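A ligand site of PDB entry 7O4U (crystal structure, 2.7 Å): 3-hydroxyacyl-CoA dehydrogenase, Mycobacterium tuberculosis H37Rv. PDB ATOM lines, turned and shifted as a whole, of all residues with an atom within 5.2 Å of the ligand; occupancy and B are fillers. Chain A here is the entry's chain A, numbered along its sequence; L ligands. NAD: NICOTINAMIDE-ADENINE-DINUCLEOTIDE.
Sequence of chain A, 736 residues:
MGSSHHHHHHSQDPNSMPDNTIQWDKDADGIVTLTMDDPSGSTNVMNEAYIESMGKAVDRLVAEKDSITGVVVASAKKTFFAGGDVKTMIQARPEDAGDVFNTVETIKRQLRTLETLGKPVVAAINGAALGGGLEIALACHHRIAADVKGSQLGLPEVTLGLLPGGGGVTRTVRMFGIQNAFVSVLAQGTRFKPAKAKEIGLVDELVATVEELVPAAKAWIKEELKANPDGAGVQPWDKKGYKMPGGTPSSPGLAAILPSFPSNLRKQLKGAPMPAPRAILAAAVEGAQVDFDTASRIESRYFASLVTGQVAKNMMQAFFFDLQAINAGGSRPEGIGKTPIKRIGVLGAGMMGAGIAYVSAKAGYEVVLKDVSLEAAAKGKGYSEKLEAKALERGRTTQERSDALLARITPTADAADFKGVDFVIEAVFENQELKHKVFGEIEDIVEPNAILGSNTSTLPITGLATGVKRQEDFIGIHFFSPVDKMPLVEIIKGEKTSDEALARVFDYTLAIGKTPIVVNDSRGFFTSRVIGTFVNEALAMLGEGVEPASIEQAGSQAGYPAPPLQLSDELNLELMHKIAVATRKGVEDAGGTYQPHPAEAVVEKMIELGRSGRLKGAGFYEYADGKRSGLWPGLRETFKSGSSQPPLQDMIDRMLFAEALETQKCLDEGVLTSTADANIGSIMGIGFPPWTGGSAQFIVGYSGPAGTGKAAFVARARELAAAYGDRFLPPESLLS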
ATOM      1  N   LEU A 347      -1.268  10.898  23.497  1.00  0.00           N
ATOM      2  CA  LEU A 347      -0.231  11.784  24.030  1.00  0.00           C
ATOM      3  C   LEU A 347      -0.879  13.104  24.428  1.00  0.00           C
ATOM      4  O   LEU A 347      -1.139  13.957  23.578  1.00  0.00           O
ATOM      5  CB  LEU A 347       0.884  11.984  23.006  1.00  0.00           C
ATOM      6  CG  LEU A 347       1.657  10.725  22.613  1.00  0.00           C
ATOM      7  CD1 LEU A 347       2.471  10.959  21.353  1.00  0.00           C
ATOM      8  CD2 LEU A 347       2.545  10.279  23.760  1.00  0.00           C
ATOM      9  N   GLY A 348      -1.138  13.274  25.716  1.00  0.00           N
ATOM     10  CA  GLY A 348      -1.735  14.496  26.211  1.00  0.00           C
ATOM     11  C   GLY A 348      -3.190  14.341  26.589  1.00  0.00           C
ATOM     12  O   GLY A 348      -4.069  14.316  25.718  1.00  0.00           O
ATOM     13  N   ALA A 349      -3.479  14.246  27.885  1.00  0.00           N
ATOM     14  CA  ALA A 349      -4.835  14.078  28.398  1.00  0.00           C
ATOM     15  C   ALA A 349      -5.381  15.436  28.807  1.00  0.00           C
ATOM     16  O   ALA A 349      -4.903  16.039  29.778  1.00  0.00           O
ATOM     17  CB  ALA A 349      -4.864  13.094  29.561  1.00  0.00           C
ATOM     18  N   GLY A 350      -6.382  15.916  28.076  1.00  0.00           N
ATOM     19  CA  GLY A 350      -7.013  17.181  28.398  1.00  0.00           C
ATOM     20  C   GLY A 350      -8.500  17.157  28.132  1.00  0.00           C
ATOM     21  O   GLY A 350      -9.136  16.111  28.293  1.00  0.00           O
ATOM     22  N   MET A 351      -9.070  18.285  27.723  1.00  0.00           N
ATOM     23  CA  MET A 351     -10.487  18.318  27.367  1.00  0.00           C
ATOM     24  C   MET A 351     -10.769  17.411  26.175  1.00  0.00           C
ATOM     25  O   MET A 351     -11.896  16.928  26.013  1.00  0.00           O
ATOM     26  CB  MET A 351     -10.934  19.743  27.082  1.00  0.00           C
ATOM     27  CG  MET A 351     -12.438  19.924  26.990  1.00  0.00           C
ATOM     28  SD  MET A 351     -12.930  21.612  26.580  1.00  0.00           S
ATOM     29  CE  MET A 351     -14.703  21.518  26.766  1.00  0.00           C
ATOM     30  N   MET A 352      -9.760  17.179  25.336  1.00  0.00           N
ATOM     31  CA  MET A 352      -9.866  16.295  24.188  1.00  0.00           C
ATOM     32  C   MET A 352      -9.156  14.966  24.394  1.00  0.00           C
ATOM     33  O   MET A 352      -9.713  13.922  24.053  1.00  0.00           O
ATOM     34  CB  MET A 352      -9.288  16.984  22.949  1.00  0.00           C
ATOM     35  CG  MET A 352      -9.988  18.287  22.583  1.00  0.00           C
ATOM     36  SD  MET A 352     -11.325  18.043  21.398  1.00  0.00           S
ATOM     37  CE  MET A 352     -10.389  17.798  19.901  1.00  0.00           C
ATOM     38  N   GLY A 353      -7.936  14.988  24.953  1.00  0.00           N
ATOM     39  CA  GLY A 353      -7.189  13.760  25.118  1.00  0.00           C
ATOM     40  C   GLY A 353      -7.897  12.752  26.001  1.00  0.00           C
ATOM     41  O   GLY A 353      -8.015  11.567  25.661  1.00  0.00           O
ATOM     42  N   LYS A 370      -0.896   8.801  28.269  1.00  0.00           N
ATOM     43  CA  LYS A 370       0.335   9.393  28.773  1.00  0.00           C
ATOM     44  C   LYS A 370       0.153  10.893  28.933  1.00  0.00           C
ATOM     45  O   LYS A 370      -0.545  11.550  28.163  1.00  0.00           O
ATOM     46  CB  LYS A 370       1.525   9.107  27.849  1.00  0.00           C
ATOM     47  CG  LYS A 370       2.872   9.486  28.450  1.00  0.00           C
ATOM     48  CD  LYS A 370       4.005   9.367  27.448  1.00  0.00           C
ATOM     49  CE  LYS A 370       5.324   9.822  28.055  1.00  0.00           C
ATOM     50  NZ  LYS A 370       6.440   9.767  27.075  1.00  0.00           N
ATOM     51  N   ASP A 371       0.810  11.438  29.962  1.00  0.00           N
ATOM     52  CA  ASP A 371       0.831  12.870  30.205  1.00  0.00           C
ATOM     53  C   ASP A 371       2.162  13.199  30.896  1.00  0.00           C
ATOM     54  O   ASP A 371       3.045  12.344  31.023  1.00  0.00           O
ATOM     55  CB  ASP A 371      -0.395  13.294  31.019  1.00  0.00           C
ATOM     56  CG  ASP A 371      -0.837  14.707  30.705  1.00  0.00           C
ATOM     57  OD1 ASP A 371      -0.031  15.642  30.901  1.00  0.00           O
ATOM     58  OD2 ASP A 371      -1.987  14.890  30.249  1.00  0.00           O
ATOM     59  N   VAL A 372       2.295  14.449  31.348  1.00  0.00           N
ATOM     60  CA  VAL A 372       3.566  14.886  31.926  1.00  0.00           C
ATOM     61  C   VAL A 372       3.871  14.117  33.211  1.00  0.00           C
ATOM     62  O   VAL A 372       4.968  13.571  33.384  1.00  0.00           O
ATOM     63  CB  VAL A 372       3.552  16.410  32.167  1.00  0.00           C
ATOM     64  CG1 VAL A 372       3.779  17.156  30.860  1.00  0.00           C
ATOM     65  CG2 VAL A 372       2.245  16.850  32.806  1.00  0.00           C
ATOM     66  N   ALA A 376      -1.342  13.478  36.356  1.00  0.00           N
ATOM     67  CA  ALA A 376      -2.036  14.130  35.250  1.00  0.00           C
ATOM     68  C   ALA A 376      -2.608  13.114  34.265  1.00  0.00           C
ATOM     69  O   ALA A 376      -3.628  13.379  33.627  1.00  0.00           O
ATOM     70  CB  ALA A 376      -1.098  15.098  34.523  1.00  0.00           C
ATOM     71  N   GLU A 426      -1.929  12.142  19.147  1.00  0.00           N
ATOM     72  CA  GLU A 426      -1.342  13.225  19.927  1.00  0.00           C
ATOM     73  C   GLU A 426      -2.383  14.278  20.266  1.00  0.00           C
ATOM     74  O   GLU A 426      -3.203  14.652  19.421  1.00  0.00           O
ATOM     75  CB  GLU A 426      -0.174  13.850  19.161  1.00  0.00           C
ATOM     76  CG  GLU A 426       0.301  15.198  19.696  1.00  0.00           C
ATOM     77  CD  GLU A 426      -0.439  16.380  19.090  1.00  0.00           C
ATOM     78  OE1 GLU A 426      -0.752  16.328  17.879  1.00  0.00           O
ATOM     79  OE2 GLU A 426      -0.728  17.345  19.823  1.00  0.00           O
ATOM     80  N   ALA A 427      -2.338  14.784  21.503  1.00  0.00           N
ATOM     81  CA  ALA A 427      -3.263  15.822  21.928  1.00  0.00           C
ATOM     82  C   ALA A 427      -2.614  16.722  22.971  1.00  0.00           C
ATOM     83  O   ALA A 427      -3.253  17.163  23.930  1.00  0.00           O
ATOM     84  CB  ALA A 427      -4.560  15.216  22.480  1.00  0.00           C
ATOM     85  N   VAL A 428      -1.330  17.029  22.784  1.00  0.00           N
ATOM     86  CA  VAL A 428      -0.582  17.868  23.720  1.00  0.00           C
ATOM     87  C   VAL A 428      -0.881  19.331  23.417  1.00  0.00           C
ATOM     88  O   VAL A 428      -1.731  19.641  22.579  1.00  0.00           O
ATOM     89  CB  VAL A 428       0.927  17.583  23.652  1.00  0.00           C
ATOM     90  CG1 VAL A 428       1.202  16.117  23.949  1.00  0.00           C
ATOM     91  CG2 VAL A 428       1.475  17.964  22.282  1.00  0.00           C
ATOM     92  N   PHE A 429      -0.182  20.243  24.108  1.00  0.00           N
ATOM     93  CA  PHE A 429      -0.327  21.657  23.835  1.00  0.00           C
ATOM     94  C   PHE A 429      -0.032  21.954  22.362  1.00  0.00           C
ATOM     95  O   PHE A 429       0.891  21.388  21.777  1.00  0.00           O
ATOM     96  CB  PHE A 429       0.617  22.472  24.726  1.00  0.00           C
ATOM     97  CG  PHE A 429       0.249  22.463  26.179  1.00  0.00           C
ATOM     98  CD1 PHE A 429      -1.071  22.334  26.582  1.00  0.00           C
ATOM     99  CD2 PHE A 429       1.234  22.579  27.159  1.00  0.00           C
ATOM    100  CE1 PHE A 429      -1.405  22.336  27.921  1.00  0.00           C
ATOM    101  CE2 PHE A 429       0.895  22.569  28.504  1.00  0.00           C
ATOM    102  CZ  PHE A 429      -0.423  22.442  28.883  1.00  0.00           C
ATOM    103  N   GLU A 430      -0.835  22.845  21.772  1.00  0.00           N
ATOM    104  CA  GLU A 430      -0.680  23.183  20.363  1.00  0.00           C
ATOM    105  C   GLU A 430       0.587  24.014  20.186  1.00  0.00           C
ATOM    106  O   GLU A 430       0.575  25.236  20.079  1.00  0.00           O
ATOM    107  CB  GLU A 430      -1.903  23.929  19.833  1.00  0.00           C
ATOM    108  CG  GLU A 430      -1.901  24.107  18.329  1.00  0.00           C
ATOM    109  CD  GLU A 430      -3.196  24.663  17.802  1.00  0.00           C
ATOM    110  OE1 GLU A 430      -3.962  25.250  18.598  1.00  0.00           O
ATOM    111  OE2 GLU A 430      -3.460  24.509  16.586  1.00  0.00           O
ATOM    112  N   LEU A 434       7.046  21.500  20.250  1.00  0.00           N
ATOM    113  CA  LEU A 434       6.731  20.531  21.291  1.00  0.00           C
ATOM    114  C   LEU A 434       6.280  19.198  20.685  1.00  0.00           C
ATOM    115  O   LEU A 434       6.728  18.138  21.142  1.00  0.00           O
ATOM    116  CB  LEU A 434       5.638  21.083  22.210  1.00  0.00           C
ATOM    117  CG  LEU A 434       5.172  20.199  23.362  1.00  0.00           C
ATOM    118  CD1 LEU A 434       6.290  19.962  24.366  1.00  0.00           C
ATOM    119  CD2 LEU A 434       3.950  20.808  24.043  1.00  0.00           C
ATOM    120  N   LYS A 435       5.434  19.242  19.664  1.00  0.00           N
ATOM    121  CA  LYS A 435       4.939  18.017  19.048  1.00  0.00           C
ATOM    122  C   LYS A 435       6.056  17.249  18.346  1.00  0.00           C
ATOM    123  O   LYS A 435       6.007  16.013  18.271  1.00  0.00           O
ATOM    124  CB  LYS A 435       3.809  18.334  18.067  1.00  0.00           C
ATOM    125  CG  LYS A 435       2.605  18.970  18.731  1.00  0.00           C
ATOM    126  CD  LYS A 435       1.656  19.567  17.702  1.00  0.00           C
ATOM    127  CE  LYS A 435       0.585  20.401  18.383  1.00  0.00           C
ATOM    128  NZ  LYS A 435      -0.304  19.583  19.249  1.00  0.00           N
ATOM    129  N   VAL A 438       7.389  15.414  21.354  1.00  0.00           N
ATOM    130  CA  VAL A 438       6.504  14.394  21.918  1.00  0.00           C
ATOM    131  C   VAL A 438       6.569  13.122  21.080  1.00  0.00           C
ATOM    132  O   VAL A 438       6.557  12.002  21.609  1.00  0.00           O
ATOM    133  CB  VAL A 438       5.062  14.928  22.031  1.00  0.00           C
ATOM    134  CG1 VAL A 438       4.148  13.868  22.598  1.00  0.00           C
ATOM    135  CG2 VAL A 438       5.031  16.174  22.903  1.00  0.00           C
ATOM    136  N   ASN A 455      -3.713  15.590  16.548  1.00  0.00           N
ATOM    137  CA  ASN A 455      -4.970  16.311  16.748  1.00  0.00           C
ATOM    138  C   ASN A 455      -4.617  17.788  16.956  1.00  0.00           C
ATOM    139  O   ASN A 455      -4.405  18.235  18.089  1.00  0.00           O
ATOM    140  CB  ASN A 455      -5.750  15.742  17.932  1.00  0.00           C
ATOM    141  CG  ASN A 455      -7.113  16.391  18.107  1.00  0.00           C
ATOM    142  OD1 ASN A 455      -8.138  15.801  17.796  1.00  0.00           O
ATOM    143  ND2 ASN A 455      -7.121  17.614  18.640  1.00  0.00           N
ATOM    144  N   THR A 456      -4.525  18.530  15.867  1.00  0.00           N
ATOM    145  CA  THR A 456      -4.224  19.948  15.895  1.00  0.00           C
ATOM    146  C   THR A 456      -5.358  20.735  15.247  1.00  0.00           C
ATOM    147  O   THR A 456      -6.007  20.253  14.309  1.00  0.00           O
ATOM    148  CB  THR A 456      -2.909  20.269  15.182  1.00  0.00           C
ATOM    149  OG1 THR A 456      -2.964  19.780  13.842  1.00  0.00           O
ATOM    150  CG2 THR A 456      -1.765  19.613  15.903  1.00  0.00           C
ATOM    151  N   SER A 457      -5.587  21.942  15.748  1.00  0.00           N
ATOM    152  CA  SER A 457      -6.689  22.766  15.261  1.00  0.00           C
ATOM    153  C   SER A 457      -6.335  23.492  13.972  1.00  0.00           C
ATOM    154  O   SER A 457      -7.155  23.567  13.057  1.00  0.00           O
ATOM    155  CB  SER A 457      -7.126  23.759  16.336  1.00  0.00           C
ATOM    156  OG  SER A 457      -6.042  24.564  16.758  1.00  0.00           O
ATOM    157  N   HIS A 478      -8.421  15.389  13.479  1.00  0.00           N
ATOM    158  CA  HIS A 478      -9.002  16.491  14.240  1.00  0.00           C
ATOM    159  C   HIS A 478     -10.356  16.074  14.805  1.00  0.00           C
ATOM    160  O   HIS A 478     -11.285  15.812  14.044  1.00  0.00           O
ATOM    161  CB  HIS A 478      -9.150  17.736  13.368  1.00  0.00           C
ATOM    162  CG  HIS A 478      -9.703  18.912  14.094  1.00  0.00           C
ATOM    163  ND1 HIS A 478     -10.819  19.600  13.676  1.00  0.00           N
ATOM    164  CD2 HIS A 478      -9.302  19.521  15.235  1.00  0.00           C
ATOM    165  CE1 HIS A 478     -11.078  20.583  14.511  1.00  0.00           C
ATOM    166  NE2 HIS A 478     -10.170  20.560  15.477  1.00  0.00           N
ATOM    167  N   PHE A 479     -10.452  16.003  16.131  1.00  0.00           N
ATOM    168  CA  PHE A 479     -11.699  15.747  16.821  1.00  0.00           C
ATOM    169  C   PHE A 479     -12.405  17.056  17.139  1.00  0.00           C
ATOM    170  O   PHE A 479     -11.950  18.149  16.777  1.00  0.00           O
ATOM    171  CB  PHE A 479     -11.451  14.943  18.099  1.00  0.00           C
ATOM    172  CG  PHE A 479     -11.126  13.497  17.864  1.00  0.00           C
ATOM    173  CD1 PHE A 479      -9.825  13.094  17.623  1.00  0.00           C
ATOM    174  CD2 PHE A 479     -12.121  12.538  17.905  1.00  0.00           C
ATOM    175  CE1 PHE A 479      -9.524  11.759  17.408  1.00  0.00           C
ATOM    176  CE2 PHE A 479     -11.832  11.213  17.698  1.00  0.00           C
ATOM    177  CZ  PHE A 479     -10.527  10.821  17.450  1.00  0.00           C
ATOM    178  N   SER A 481     -14.710  18.962  20.507  1.00  0.00           N
ATOM    179  CA  SER A 481     -15.026  18.883  21.937  1.00  0.00           C
ATOM    180  C   SER A 481     -16.478  19.262  22.200  1.00  0.00           C
ATOM    181  O   SER A 481     -16.995  20.195  21.571  1.00  0.00           O
ATOM    182  CB  SER A 481     -14.104  19.791  22.740  1.00  0.00           C
ATOM    183  OG  SER A 481     -14.323  19.640  24.141  1.00  0.00           O
HETATM  184  PA  NAD L   1      -5.330  21.155  26.989  1.00  0.00           P
HETATM  185  O1A NAD L   1      -4.596  22.222  26.243  1.00  0.00           O
HETATM  186  O2A NAD L   1      -6.465  21.553  27.876  1.00  0.00           O
HETATM  187  O5B NAD L   1      -4.296  20.260  27.808  1.00  0.00           O
HETATM  188  C5B NAD L   1      -3.255  19.569  27.070  1.00  0.00           C
HETATM  189  C4B NAD L   1      -2.657  18.503  27.941  1.00  0.00           C
HETATM  190  O4B NAD L   1      -1.359  18.106  27.418  1.00  0.00           O
HETATM  191  C3B NAD L   1      -2.424  18.860  29.416  1.00  0.00           C
HETATM  192  O3B NAD L   1      -3.036  17.879  30.247  1.00  0.00           O
HETATM  193  C2B NAD L   1      -0.900  18.791  29.557  1.00  0.00           C
HETATM  194  O2B NAD L   1      -0.444  18.470  30.862  1.00  0.00           O
HETATM  195  C1B NAD L   1      -0.563  17.732  28.511  1.00  0.00           C
HETATM  196  N9A NAD L   1       0.836  17.718  28.111  1.00  0.00           N
HETATM  197  C8A NAD L   1       1.685  18.795  28.043  1.00  0.00           C
HETATM  198  N7A NAD L   1       2.900  18.487  27.665  1.00  0.00           N
HETATM  199  C5A NAD L   1       2.856  17.112  27.485  1.00  0.00           C
HETATM  200  C6A NAD L   1       3.830  16.178  27.086  1.00  0.00           C
HETATM  201  N6A NAD L   1       5.090  16.507  26.795  1.00  0.00           N
HETATM  202  N1A NAD L   1       3.467  14.876  27.010  1.00  0.00           N
HETATM  203  C2A NAD L   1       2.194  14.557  27.308  1.00  0.00           C
HETATM  204  N3A NAD L   1       1.194  15.343  27.693  1.00  0.00           N
HETATM  205  C4A NAD L   1       1.595  16.626  27.763  1.00  0.00           C
HETATM  206  O3  NAD L   1      -5.846  20.051  25.943  1.00  0.00           O
HETATM  207  PN  NAD L   1      -6.796  20.090  24.659  1.00  0.00           P
HETATM  208  O1N NAD L   1      -7.897  19.111  24.854  1.00  0.00           O
HETATM  209  O2N NAD L   1      -7.137  21.517  24.358  1.00  0.00           O
HETATM  210  O5D NAD L   1      -5.793  19.542  23.528  1.00  0.00           O
HETATM  211  C5D NAD L   1      -6.374  19.212  22.247  1.00  0.00           C
HETATM  212  C4D NAD L   1      -5.358  19.371  21.155  1.00  0.00           C
HETATM  213  O4D NAD L   1      -6.062  19.501  19.901  1.00  0.00           O
HETATM  214  C3D NAD L   1      -4.521  20.655  21.213  1.00  0.00           C
HETATM  215  O3D NAD L   1      -3.416  20.561  20.316  1.00  0.00           O
HETATM  216  C2D NAD L   1      -5.552  21.664  20.713  1.00  0.00           C
HETATM  217  O2D NAD L   1      -5.009  22.879  20.221  1.00  0.00           O
HETATM  218  C1D NAD L   1      -6.336  20.890  19.649  1.00  0.00           C
HETATM  219  N1N NAD L   1      -7.808  21.117  19.759  1.00  0.00           N
HETATM  220  C2N NAD L   1      -8.366  21.492  20.967  1.00  0.00           C
HETATM  221  C3N NAD L   1      -9.743  21.606  21.096  1.00  0.00           C
HETATM  222  C7N NAD L   1     -10.311  21.872  22.473  1.00  0.00           C
HETATM  223  O7N NAD L   1     -11.530  21.969  22.614  1.00  0.00           O
HETATM  224  N7N NAD L   1      -9.451  21.979  23.475  1.00  0.00           N
HETATM  225  C4N NAD L   1     -10.536  21.475  19.971  1.00  0.00           C
HETATM  226  C5N NAD L   1      -9.966  21.176  18.752  1.00  0.00           C
HETATM  227  C6N NAD L   1      -8.607  20.978  18.675  1.00  0.00           C
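O of Ala 349 sits at hydrogen-bond distance from O3B of the ligand. The backbone NH (N) of Met 351 is in hydrogen-bond range of an oxygen (O1N) of the ligand (3.2 Å). The backbone carbonyl oxygen (O) of Asn 455 sits at hydrogen-bond distance from an oxygen (O3D) of the ligand, 3.4 Å away. The side-chain carboxylate (OE1) of Glu 430 sits at hydrogen-bond distance from an oxygen (O2D) of the ligand, 3.1 Å away. NZ of Lys 435 is in hydrogen-bond range of O3D of the ligand (3.4 Å). The backbone NH of Met 352 lies within hydrogen-bond range of an oxygen (O1N) of the ligand. An oxygen (O2B) of the ligand sits at hydrogen-bond distance from the side-chain carboxylate (OD1) of Asp 371, 2.9 Å away. The side-chain amide nitrogen (ND2) of Asn 455 is in hydrogen-bond range of an oxygen (O4D) of the ligand, at 2.5 Å. The backbone carbonyl oxygen (O) of Val 428 lies within hydrogen-bond range of an oxygen (O3D) of the ligand, 3.0 Å away.
N of Val 428 is in hydrogen-bond range of O of Leu 347 (3.2 Å). N of Ser 481 sits close to SD of Met 352 (3.6 Å). The backbone NH of Ala 349 is in hydrogen-bond range of the side-chain carboxylate of Asp 371 (2.9 Å). N of Gly 348 sits at hydrogen-bond distance from O of Lys 370, at 3.1 Å. NZ of Lys 435 is in hydrogen-bond range of O of Phe 429. O of Leu 347 sits at hydrogen-bond distance from N of Ala 427, 2.5 Å away. N of Phe 479 is in hydrogen-bond range of OD1 of Asn 455 (2.9 Å). NZ of Lys 435 lies within salt-bridge range of OE1 of Glu 426, at 3.6 Å.
CA of Gly 348 touches N3A of the ligand, 3.4 Å away. Gly 350 touches the ligand. Val 372 touches the ligand (CG1 to C5A, 3.5 Å). O of Ala 427 touches O5D of the ligand, at 3.5 Å. CE1 of Phe 429 touches C5B of the ligand, at 3.4 Å. Val 438 touches the ligand (CG2 to N6A, 3.9 Å). Ser 457 touches the ligand. His 478 touches the ligand. CB of Ser 481 touches O7N of the ligand, 3.4 Å away. Hydrophobic or aromatic side chains that line the ligand: Met 351, Met 352, Val 372, Val 428, Phe 429, Val 438 and His 478. Of the 25 residues printed, 17 come within 4 Å of the ligand. Along chain A the residues within 4 Å of the ligand span positions 348 to 481. The nearest printed residue that does not touch the ligand is Phe 479 (4.1 Å).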
